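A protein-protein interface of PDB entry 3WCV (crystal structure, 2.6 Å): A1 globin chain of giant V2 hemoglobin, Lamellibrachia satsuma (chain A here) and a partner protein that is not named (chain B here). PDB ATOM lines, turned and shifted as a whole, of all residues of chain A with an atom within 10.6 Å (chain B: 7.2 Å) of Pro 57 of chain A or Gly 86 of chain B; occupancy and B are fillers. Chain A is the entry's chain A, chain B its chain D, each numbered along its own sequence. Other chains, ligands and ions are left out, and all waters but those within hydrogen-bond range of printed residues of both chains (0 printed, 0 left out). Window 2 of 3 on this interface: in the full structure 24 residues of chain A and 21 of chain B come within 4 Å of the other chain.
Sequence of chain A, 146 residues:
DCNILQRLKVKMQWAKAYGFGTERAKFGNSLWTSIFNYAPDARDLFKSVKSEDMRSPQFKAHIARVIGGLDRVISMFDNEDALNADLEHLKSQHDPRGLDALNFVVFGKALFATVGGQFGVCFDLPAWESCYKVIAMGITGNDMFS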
ATOM      1  N   ALA A  25      12.116   2.521 -10.601  1.00  0.00           N
ATOM      2  CA  ALA A  25      11.612   1.419 -11.407  1.00  0.00           C
ATOM      3  C   ALA A  25      10.959   0.357 -10.511  1.00  0.00           C
ATOM      4  O   ALA A  25       9.906  -0.172 -10.837  1.00  0.00           O
ATOM      5  CB  ALA A  25      12.750   0.813 -12.233  1.00  0.00           C
ATOM      6  N   ASN A  29       7.346  -0.972 -10.797  1.00  0.00           N
ATOM      7  CA  ASN A  29       7.008  -2.374 -11.007  1.00  0.00           C
ATOM      8  C   ASN A  29       5.991  -2.901  -9.989  1.00  0.00           C
ATOM      9  O   ASN A  29       5.117  -3.712 -10.336  1.00  0.00           O
ATOM     10  CB  ASN A  29       8.271  -3.252 -11.005  1.00  0.00           C
ATOM     11  CG  ASN A  29       7.942  -4.741 -11.153  1.00  0.00           C
ATOM     12  OD1 ASN A  29       7.667  -5.423 -10.160  1.00  0.00           O
ATOM     13  ND2 ASN A  29       7.937  -5.243 -12.401  1.00  0.00           N
ATOM     14  N   PHE A  46      -3.074  -3.832 -22.140  1.00  0.00           N
ATOM     15  CA  PHE A  46      -1.734  -3.322 -22.408  1.00  0.00           C
ATOM     16  C   PHE A  46      -0.854  -4.132 -23.354  1.00  0.00           C
ATOM     17  O   PHE A  46       0.379  -4.139 -23.214  1.00  0.00           O
ATOM     18  CB  PHE A  46      -1.019  -3.116 -21.075  1.00  0.00           C
ATOM     19  CG  PHE A  46      -1.713  -2.142 -20.175  1.00  0.00           C
ATOM     20  CD1 PHE A  46      -1.398  -0.779 -20.216  1.00  0.00           C
ATOM     21  CD2 PHE A  46      -2.721  -2.577 -19.309  1.00  0.00           C
ATOM     22  CE1 PHE A  46      -2.085   0.133 -19.403  1.00  0.00           C
ATOM     23  CE2 PHE A  46      -3.415  -1.676 -18.493  1.00  0.00           C
ATOM     24  CZ  PHE A  46      -3.101  -0.319 -18.537  1.00  0.00           C
ATOM     25  N   SER A  48      -0.261  -3.424 -26.298  1.00  0.00           N
ATOM     26  CA  SER A  48       0.494  -2.446 -27.073  1.00  0.00           C
ATOM     27  C   SER A  48       1.856  -2.119 -26.443  1.00  0.00           C
ATOM     28  O   SER A  48       2.754  -1.625 -27.117  1.00  0.00           O
ATOM     29  CB  SER A  48      -0.315  -1.148 -27.226  1.00  0.00           C
ATOM     30  OG  SER A  48      -0.761  -0.642 -25.971  1.00  0.00           O
ATOM     31  N   VAL A  49       2.002  -2.374 -25.147  1.00  0.00           N
ATOM     32  CA  VAL A  49       3.263  -2.103 -24.477  1.00  0.00           C
ATOM     33  C   VAL A  49       3.881  -3.376 -23.918  1.00  0.00           C
ATOM     34  O   VAL A  49       4.717  -3.337 -23.012  1.00  0.00           O
ATOM     35  CB  VAL A  49       3.110  -1.042 -23.347  1.00  0.00           C
ATOM     36  CG1 VAL A  49       3.066   0.333 -23.951  1.00  0.00           C
ATOM     37  CG2 VAL A  49       1.857  -1.303 -22.533  1.00  0.00           C
ATOM     38  N   LYS A  50       3.442  -4.504 -24.469  1.00  0.00           N
ATOM     39  CA  LYS A  50       3.960  -5.827 -24.125  1.00  0.00           C
ATOM     40  C   LYS A  50       3.796  -6.206 -22.655  1.00  0.00           C
ATOM     41  O   LYS A  50       4.740  -6.685 -22.029  1.00  0.00           O
ATOM     42  CB  LYS A  50       5.435  -5.901 -24.525  1.00  0.00           C
ATOM     43  CG  LYS A  50       5.929  -7.263 -25.016  1.00  0.00           C
ATOM     44  CD  LYS A  50       7.379  -7.118 -25.502  1.00  0.00           C
ATOM     45  CE  LYS A  50       7.971  -8.414 -26.037  1.00  0.00           C
ATOM     46  NZ  LYS A  50       9.422  -8.249 -26.332  1.00  0.00           N
ATOM     47  N   SER A  51       2.589  -5.995 -22.120  1.00  0.00           N
ATOM     48  CA  SER A  51       2.277  -6.319 -20.726  1.00  0.00           C
ATOM     49  C   SER A  51       2.423  -7.822 -20.533  1.00  0.00           C
ATOM     50  O   SER A  51       2.442  -8.333 -19.422  1.00  0.00           O
ATOM     51  CB  SER A  51       0.843  -5.907 -20.386  1.00  0.00           C
ATOM     52  OG  SER A  51      -0.110  -6.691 -21.098  1.00  0.00           O
ATOM     53  N   GLU A  52       2.498  -8.523 -21.649  1.00  0.00           N
ATOM     54  CA  GLU A  52       2.665  -9.964 -21.671  1.00  0.00           C
ATOM     55  C   GLU A  52       3.884 -10.353 -20.815  1.00  0.00           C
ATOM     56  O   GLU A  52       3.923 -11.409 -20.191  1.00  0.00           O
ATOM     57  CB  GLU A  52       2.882 -10.390 -23.122  1.00  0.00           C
ATOM     58  CG  GLU A  52       2.408  -9.311 -24.104  1.00  0.00           C
ATOM     59  CD  GLU A  52       3.000  -9.463 -25.497  1.00  0.00           C
ATOM     60  OE1 GLU A  52       2.735  -8.600 -26.367  1.00  0.00           O
ATOM     61  OE2 GLU A  52       3.734 -10.451 -25.724  1.00  0.00           O
ATOM     62  N   ASP A  53       4.884  -9.480 -20.794  1.00  0.00           N
ATOM     63  CA  ASP A  53       6.105  -9.719 -20.056  1.00  0.00           C
ATOM     64  C   ASP A  53       6.512  -8.424 -19.384  1.00  0.00           C
ATOM     65  O   ASP A  53       7.100  -7.550 -20.009  1.00  0.00           O
ATOM     66  CB  ASP A  53       7.186 -10.197 -21.027  1.00  0.00           C
ATOM     67  CG  ASP A  53       8.553 -10.267 -20.397  1.00  0.00           C
ATOM     68  OD1 ASP A  53       8.660 -10.709 -19.236  1.00  0.00           O
ATOM     69  OD2 ASP A  53       9.532  -9.891 -21.070  1.00  0.00           O
ATOM     70  N   MET A  54       6.202  -8.316 -18.101  1.00  0.00           N
ATOM     71  CA  MET A  54       6.495  -7.116 -17.341  1.00  0.00           C
ATOM     72  C   MET A  54       7.949  -6.734 -17.205  1.00  0.00           C
ATOM     73  O   MET A  54       8.254  -5.629 -16.804  1.00  0.00           O
ATOM     74  CB  MET A  54       5.866  -7.238 -15.970  1.00  0.00           C
ATOM     75  CG  MET A  54       4.361  -7.161 -16.014  1.00  0.00           C
ATOM     76  SD  MET A  54       3.720  -7.262 -14.344  1.00  0.00           S
ATOM     77  CE  MET A  54       3.966  -5.565 -13.812  1.00  0.00           C
ATOM     78  N   ARG A  55       8.841  -7.641 -17.542  1.00  0.00           N
ATOM     79  CA  ARG A  55      10.266  -7.366 -17.421  1.00  0.00           C
ATOM     80  C   ARG A  55      10.818  -6.873 -18.746  1.00  0.00           C
ATOM     81  O   ARG A  55      11.968  -6.472 -18.834  1.00  0.00           O
ATOM     82  CB  ARG A  55      11.002  -8.626 -16.954  1.00  0.00           C
ATOM     83  CG  ARG A  55      10.146  -9.905 -17.030  1.00  0.00           C
ATOM     84  CD  ARG A  55      10.970 -11.180 -16.900  1.00  0.00           C
ATOM     85  NE  ARG A  55      11.587 -11.313 -15.583  1.00  0.00           N
ATOM     86  CZ  ARG A  55      12.541 -12.193 -15.293  1.00  0.00           C
ATOM     87  NH1 ARG A  55      13.047 -12.248 -14.066  1.00  0.00           N
ATOM     88  NH2 ARG A  55      13.000 -13.011 -16.233  1.00  0.00           N
ATOM     89  N   SER A  56       9.980  -6.885 -19.768  1.00  0.00           N
ATOM     90  CA  SER A  56      10.373  -6.431 -21.093  1.00  0.00           C
ATOM     91  C   SER A  56      10.591  -4.916 -21.149  1.00  0.00           C
ATOM     92  O   SER A  56       9.900  -4.144 -20.493  1.00  0.00           O
ATOM     93  CB  SER A  56       9.294  -6.799 -22.097  1.00  0.00           C
ATOM     94  OG  SER A  56       8.221  -5.874 -22.025  1.00  0.00           O
ATOM     95  N   PRO A  57      11.552  -4.465 -21.965  1.00  0.00           N
ATOM     96  CA  PRO A  57      11.800  -3.023 -22.055  1.00  0.00           C
ATOM     97  C   PRO A  57      10.591  -2.220 -22.514  1.00  0.00           C
ATOM     98  O   PRO A  57      10.413  -1.073 -22.108  1.00  0.00           O
ATOM     99  CB  PRO A  57      12.983  -2.931 -23.026  1.00  0.00           C
ATOM    100  CG  PRO A  57      12.789  -4.153 -23.898  1.00  0.00           C
ATOM    101  CD  PRO A  57      12.417  -5.222 -22.891  1.00  0.00           C
ATOM    102  N   GLN A  58       9.756  -2.811 -23.361  1.00  0.00           N
ATOM    103  CA  GLN A  58       8.565  -2.117 -23.832  1.00  0.00           C
ATOM    104  C   GLN A  58       7.668  -1.752 -22.652  1.00  0.00           C
ATOM    105  O   GLN A  58       7.241  -0.606 -22.538  1.00  0.00           O
ATOM    106  CB  GLN A  58       7.781  -2.986 -24.815  1.00  0.00           C
ATOM    107  CG  GLN A  58       8.339  -2.993 -26.232  1.00  0.00           C
ATOM    108  CD  GLN A  58       9.691  -3.687 -26.348  1.00  0.00           C
ATOM    109  OE1 GLN A  58       9.885  -4.807 -25.855  1.00  0.00           O
ATOM    110  NE2 GLN A  58      10.639  -3.020 -27.016  1.00  0.00           N
ATOM    111  N   PHE A  59       7.417  -2.717 -21.766  1.00  0.00           N
ATOM    112  CA  PHE A  59       6.568  -2.476 -20.610  1.00  0.00           C
ATOM    113  C   PHE A  59       7.211  -1.611 -19.541  1.00  0.00           C
ATOM    114  O   PHE A  59       6.510  -0.906 -18.811  1.00  0.00           O
ATOM    115  CB  PHE A  59       6.121  -3.780 -19.963  1.00  0.00           C
ATOM    116  CG  PHE A  59       4.985  -3.604 -18.999  1.00  0.00           C
ATOM    117  CD1 PHE A  59       5.198  -3.608 -17.628  1.00  0.00           C
ATOM    118  CD2 PHE A  59       3.691  -3.389 -19.474  1.00  0.00           C
ATOM    119  CE1 PHE A  59       4.127  -3.397 -16.741  1.00  0.00           C
ATOM    120  CE2 PHE A  59       2.626  -3.176 -18.600  1.00  0.00           C
ATOM    121  CZ  PHE A  59       2.840  -3.180 -17.236  1.00  0.00           C
ATOM    122  N   LYS A  60       8.532  -1.683 -19.426  1.00  0.00           N
ATOM    123  CA  LYS A  60       9.254  -0.879 -18.444  1.00  0.00           C
ATOM    124  C   LYS A  60       9.198   0.582 -18.876  1.00  0.00           C
ATOM    125  O   LYS A  60       9.140   1.485 -18.044  1.00  0.00           O
ATOM    126  CB  LYS A  60      10.707  -1.327 -18.332  1.00  0.00           C
ATOM    127  CG  LYS A  60      10.937  -2.603 -17.519  1.00  0.00           C
ATOM    128  CD  LYS A  60      12.412  -2.901 -17.557  1.00  0.00           C
ATOM    129  CE  LYS A  60      12.798  -4.167 -16.859  1.00  0.00           C
ATOM    130  NZ  LYS A  60      14.252  -4.465 -17.119  1.00  0.00           N
ATOM    131  N   ALA A  61       9.215   0.805 -20.184  1.00  0.00           N
ATOM    132  CA  ALA A  61       9.131   2.158 -20.714  1.00  0.00           C
ATOM    133  C   ALA A  61       7.724   2.720 -20.369  1.00  0.00           C
ATOM    134  O   ALA A  61       7.539   3.930 -20.105  1.00  0.00           O
ATOM    135  CB  ALA A  61       9.346   2.130 -22.233  1.00  0.00           C
ATOM    136  N   HIS A  62       6.736   1.828 -20.387  1.00  0.00           N
ATOM    137  CA  HIS A  62       5.378   2.218 -20.072  1.00  0.00           C
ATOM    138  C   HIS A  62       5.288   2.581 -18.586  1.00  0.00           C
ATOM    139  O   HIS A  62       4.751   3.633 -18.215  1.00  0.00           O
ATOM    140  CB  HIS A  62       4.411   1.087 -20.382  1.00  0.00           C
ATOM    141  CG  HIS A  62       3.017   1.389 -19.955  1.00  0.00           C
ATOM    142  ND1 HIS A  62       2.252   2.360 -20.562  1.00  0.00           N
ATOM    143  CD2 HIS A  62       2.273   0.901 -18.935  1.00  0.00           C
ATOM    144  CE1 HIS A  62       1.093   2.454 -19.934  1.00  0.00           C
ATOM    145  NE2 HIS A  62       1.081   1.577 -18.943  1.00  0.00           N
ATOM    146  N   ILE A  63       5.812   1.692 -17.742  1.00  0.00           N
ATOM    147  CA  ILE A  63       5.830   1.930 -16.305  1.00  0.00           C
ATOM    148  C   ILE A  63       6.486   3.288 -16.033  1.00  0.00           C
ATOM    149  O   ILE A  63       5.947   4.106 -15.285  1.00  0.00           O
ATOM    150  CB  ILE A  63       6.619   0.829 -15.574  1.00  0.00           C
ATOM    151  CG1 ILE A  63       5.859  -0.495 -15.697  1.00  0.00           C
ATOM    152  CG2 ILE A  63       6.831   1.211 -14.111  1.00  0.00           C
ATOM    153  CD1 ILE A  63       6.529  -1.662 -15.045  1.00  0.00           C
ATOM    154  N   ALA A  64       7.625   3.529 -16.678  1.00  0.00           N
ATOM    155  CA  ALA A  64       8.361   4.777 -16.496  1.00  0.00           C
ATOM    156  C   ALA A  64       7.537   5.992 -16.927  1.00  0.00           C
ATOM    157  O   ALA A  64       7.549   7.030 -16.245  1.00  0.00           O
ATOM    158  CB  ALA A  64       9.709   4.735 -17.276  1.00  0.00           C
ATOM    159  N   ARG A  65       6.808   5.859 -18.034  1.00  0.00           N
ATOM    160  CA  ARG A  65       6.007   6.979 -18.500  1.00  0.00           C
ATOM    161  C   ARG A  65       4.873   7.288 -17.535  1.00  0.00           C
ATOM    162  O   ARG A  65       4.602   8.456 -17.234  1.00  0.00           O
ATOM    163  CB  ARG A  65       5.451   6.716 -19.906  1.00  0.00           C
ATOM    164  CG  ARG A  65       6.460   7.030 -21.011  1.00  0.00           C
ATOM    165  CD  ARG A  65       5.846   6.985 -22.403  1.00  0.00           C
ATOM    166  NE  ARG A  65       5.353   5.648 -22.792  1.00  0.00           N
ATOM    167  CZ  ARG A  65       6.089   4.673 -23.339  1.00  0.00           C
ATOM    168  NH1 ARG A  65       7.385   4.845 -23.577  1.00  0.00           N
ATOM    169  NH2 ARG A  65       5.523   3.525 -23.683  1.00  0.00           N
ATOM    170  N   PHE B   3      25.022   3.947 -25.256  1.00  0.00           N
ATOM    171  CA  PHE B   3      24.744   5.258 -24.671  1.00  0.00           C
ATOM    172  C   PHE B   3      25.938   5.951 -24.040  1.00  0.00           C
ATOM    173  O   PHE B   3      26.780   6.506 -24.745  1.00  0.00           O
ATOM    174  CB  PHE B   3      23.638   5.151 -23.629  1.00  0.00           C
ATOM    175  CG  PHE B   3      22.273   5.274 -24.208  1.00  0.00           C
ATOM    176  CD1 PHE B   3      21.497   4.151 -24.441  1.00  0.00           C
ATOM    177  CD2 PHE B   3      21.784   6.518 -24.583  1.00  0.00           C
ATOM    178  CE1 PHE B   3      20.254   4.268 -25.044  1.00  0.00           C
ATOM    179  CE2 PHE B   3      20.547   6.642 -25.186  1.00  0.00           C
ATOM    180  CZ  PHE B   3      19.780   5.516 -25.418  1.00  0.00           C
ATOM    181  N   TYR B  81      17.127   6.752 -16.535  1.00  0.00           N
ATOM    182  CA  TYR B  81      17.223   5.445 -17.156  1.00  0.00           C
ATOM    183  C   TYR B  81      18.520   5.263 -17.953  1.00  0.00           C
ATOM    184  O   TYR B  81      18.654   4.306 -18.714  1.00  0.00           O
ATOM    185  CB  TYR B  81      15.994   5.195 -18.037  1.00  0.00           C
ATOM    186  CG  TYR B  81      14.817   4.703 -17.239  1.00  0.00           C
ATOM    187  CD1 TYR B  81      14.643   3.341 -16.982  1.00  0.00           C
ATOM    188  CD2 TYR B  81      13.923   5.603 -16.668  1.00  0.00           C
ATOM    189  CE1 TYR B  81      13.604   2.883 -16.162  1.00  0.00           C
ATOM    190  CE2 TYR B  81      12.886   5.162 -15.845  1.00  0.00           C
ATOM    191  CZ  TYR B  81      12.738   3.800 -15.597  1.00  0.00           C
ATOM    192  OH  TYR B  81      11.733   3.388 -14.761  1.00  0.00           O
ATOM    193  N   ASN B  83      21.314   4.190 -17.096  1.00  0.00           N
ATOM    194  CA  ASN B  83      21.967   2.916 -16.823  1.00  0.00           C
ATOM    195  C   ASN B  83      21.063   1.708 -17.073  1.00  0.00           C
ATOM    196  O   ASN B  83      21.285   0.638 -16.508  1.00  0.00           O
ATOM    197  CB  ASN B  83      22.528   2.879 -15.386  1.00  0.00           C
ATOM    198  CG  ASN B  83      23.802   3.747 -15.221  1.00  0.00           C
ATOM    199  OD1 ASN B  83      24.711   3.704 -16.057  1.00  0.00           O
ATOM    200  ND2 ASN B  83      23.861   4.523 -14.141  1.00  0.00           N
ATOM    201  N   ASP B  84      20.038   1.878 -17.910  1.00  0.00           N
ATOM    202  CA  ASP B  84      19.142   0.774 -18.274  1.00  0.00           C
ATOM    203  C   ASP B  84      18.979   0.872 -19.782  1.00  0.00           C
ATOM    204  O   ASP B  84      17.903   1.202 -20.284  1.00  0.00           O
ATOM    205  CB  ASP B  84      17.764   0.895 -17.617  1.00  0.00           C
ATOM    206  CG  ASP B  84      16.918  -0.382 -17.784  1.00  0.00           C
ATOM    207  OD1 ASP B  84      17.042  -1.061 -18.835  1.00  0.00           O
ATOM    208  OD2 ASP B  84      16.113  -0.714 -16.879  1.00  0.00           O
ATOM    209  N   ALA B  85      20.064   0.584 -20.494  1.00  0.00           N
ATOM    210  CA  ALA B  85      20.102   0.663 -21.947  1.00  0.00           C
ATOM    211  C   ALA B  85      18.871   0.116 -22.652  1.00  0.00           C
ATOM    212  O   ALA B  85      18.348   0.742 -23.568  1.00  0.00           O
ATOM    213  CB  ALA B  85      21.352  -0.044 -22.464  1.00  0.00           C
ATOM    214  N   GLY B  86      18.412  -1.058 -22.240  1.00  0.00           N
ATOM    215  CA  GLY B  86      17.253  -1.647 -22.884  1.00  0.00           C
ATOM    216  C   GLY B  86      16.023  -0.760 -22.820  1.00  0.00           C
ATOM    217  O   GLY B  86      15.434  -0.409 -23.852  1.00  0.00           O
ATOM    218  N   THR B  87      15.639  -0.388 -21.602  1.00  0.00           N
ATOM    219  CA  THR B  87      14.454   0.434 -21.410  1.00  0.00           C
ATOM    220  C   THR B  87      14.601   1.815 -22.009  1.00  0.00           C
ATOM    221  O   THR B  87      13.652   2.345 -22.577  1.00  0.00           O
ATOM    222  CB  THR B  87      14.125   0.604 -19.932  1.00  0.00           C
ATOM    223  OG1 THR B  87      14.048  -0.680 -19.314  1.00  0.00           O
ATOM    224  CG2 THR B  87      12.795   1.307 -19.763  1.00  0.00           C
ATOM    225  N   LEU B  88      15.785   2.398 -21.886  1.00  0.00           N
ATOM    226  CA  LEU B  88      16.021   3.734 -22.412  1.00  0.00           C
ATOM    227  C   LEU B  88      15.838   3.717 -23.916  1.00  0.00           C
ATOM    228  O   LEU B  88      15.240   4.628 -24.489  1.00  0.00           O
ATOM    229  CB  LEU B  88      17.432   4.216 -22.052  1.00  0.00           C
ATOM    230  CG  LEU B  88      17.761   5.687 -22.368  1.00  0.00           C
ATOM    231  CD1 LEU B  88      16.740   6.628 -21.706  1.00  0.00           C
ATOM    232  CD2 LEU B  88      19.153   6.003 -21.874  1.00  0.00           C
ATOM    233  N   THR B  89      16.346   2.676 -24.563  1.00  0.00           N
ATOM    234  CA  THR B  89      16.206   2.579 -26.005  1.00  0.00           C
ATOM    235  C   THR B  89      14.718   2.644 -26.335  1.00  0.00           C
ATOM    236  O   THR B  89      14.292   3.408 -27.210  1.00  0.00           O
ATOM    237  CB  THR B  89      16.776   1.270 -26.520  1.00  0.00           C
ATOM    238  OG1 THR B  89      18.163   1.202 -26.188  1.00  0.00           O
ATOM    239  CG2 THR B  89      16.604   1.182 -28.025  1.00  0.00           C
ATOM    240  N   SER B  90      13.931   1.848 -25.616  1.00  0.00           N
ATOM    241  CA  SER B  90      12.492   1.815 -25.804  1.00  0.00           C
ATOM    242  C   SER B  90      11.852   3.164 -25.469  1.00  0.00           C
ATOM    243  O   SER B  90      10.939   3.610 -26.162  1.00  0.00           O
ATOM    244  CB  SER B  90      11.883   0.736 -24.925  1.00  0.00           C
ATOM    245  OG  SER B  90      10.474   0.853 -24.924  1.00  0.00           O
ATOM    246  N   LEU B  91      12.331   3.815 -24.417  1.00  0.00           N
ATOM    247  CA  LEU B  91      11.797   5.126 -24.027  1.00  0.00           C
ATOM    248  C   LEU B  91      12.077   6.194 -25.076  1.00  0.00           C
ATOM    249  O   LEU B  91      11.225   7.033 -25.369  1.00  0.00           O
ATOM    250  CB  LEU B  91      12.388   5.593 -22.689  1.00  0.00           C
ATOM    251  CG  LEU B  91      11.935   4.934 -21.375  1.00  0.00           C
ATOM    252  CD1 LEU B  91      12.770   5.505 -20.244  1.00  0.00           C
ATOM    253  CD2 LEU B  91      10.436   5.186 -21.125  1.00  0.00           C
ATOM    254  N   THR B  92      13.276   6.182 -25.643  1.00  0.00           N
ATOM    255  CA  THR B  92      13.616   7.196 -26.634  1.00  0.00           C
ATOM    256  C   THR B  92      12.909   6.932 -27.954  1.00  0.00           C
ATOM    257  O   THR B  92      12.553   7.876 -28.672  1.00  0.00           O
ATOM    258  CB  THR B  92      15.156   7.281 -26.875  1.00  0.00           C
ATOM    259  OG1 THR B  92      15.657   6.015 -27.327  1.00  0.00           O
ATOM    260  CG2 THR B  92      15.870   7.677 -25.588  1.00  0.00           C
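The backbone carbonyl oxygen of Arg 55 of chain A lies close to the side-chain amino group of Lys 60 of chain A.
The side-chain carboxylate (OD1) of Asp 84 of chain B lies within hydrogen-bond range of the side-chain hydroxyl (OG1) of Thr 87 of chain B (3.1 Å).
The side-chain hydroxyl (OG) of Ser 90 of chain B lies within hydrogen-bond range of the backbone carbonyl oxygen (O) of Pro 57 of chain A (3.4 Å).
Of chain B, only Gly 86, Thr 87 and Ser 90 come within 4 Å of Pro 57 of chain A.
Of the printed residues of chain A, Gly 86 of chain B touches Pro 57 (3.6 Å).
Asp 84 of chain B touches none of the printed residues of chain A.
No residue of chain A comes within 4 Å of Ala 85 of chain B.
Of the printed residues of chain A, Thr 87 of chain B touches Pro 57 (3.9 Å), Lys 60 (3.3 Å) and Ala 61 (3.6 Å).
No residue of chain A comes within 4 Å of Thr 89 of chain B.
Printed residues of chain B within 4 Å of Ala 25 of chain A: Tyr 81 (3.7 Å).
Of the printed residues of chain B, Ala 61 of chain A touches Thr 87 (3.6 Å), Ser 90 (3.2 Å) and Leu 91 (3.3 Å).
Of the printed residues of chain B, Arg 65 of chain A touches Leu 91 (3.9 Å).
Ser 56 of chain A touches none of the printed residues of chain B.
Ser 48 of chain A touches none of the printed residues of chain B.
The nearest residue of chain A that does not touch Gly 86 of chain B is Gln 58 of chain A (6.2 Å).
Among the printed residues, pairs that only touch across the chains: Ala 25 of chain A with Tyr 81 of chain B (3.7 Å), Pro 57 of chain A with Gly 86 of chain B (3.6 Å), Pro 57 of chain A with Thr 87 of chain B (3.9 Å), Gln 58 of chain A with Ser 90 of chain B (3.7 Å), Lys 60 of chain A with Thr 87 of chain B (3.3 Å), Ala 61 of chain A with Thr 87 of chain B (3.6 Å), Ala 61 of chain A with Ser 90 of chain B (3.2 Å), Ala 61 of chain A with Leu 91 of chain B (3.3 Å), Ala 64 of chain A with Tyr 81 of chain B (3.5 Å), Ala 64 of chain A with Leu 91 of chain B (3.9 Å) and Arg 65 of chain A with Leu 91 of chain B (3.9 Å).
Of the 12 printed residues of chain B, 5 touch a printed residue of chain A.
Along chain B the printed residues that touch a printed residue of chain A span positions 81 to 91.
Printed residues of chain A that touch a printed residue of chain B: Ala 25, Pro 57, Gln 58, Lys 60, Ala 61, Ala 64 and Arg 65.
Hydrophobic or aromatic side chains of chain A that line the printed part of chain B: Ala 25, Pro 57, Ala 61 and Ala 64.
Along chain A the printed residues that touch a printed residue of chain B span positions 25 to 65.
Among the printed residues, 12 pairs touch across the chains.
Among the printed residues, no Asp or Glu carboxylate lies within 4 Å of a Lys or Arg side-chain nitrogen of the other chain.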
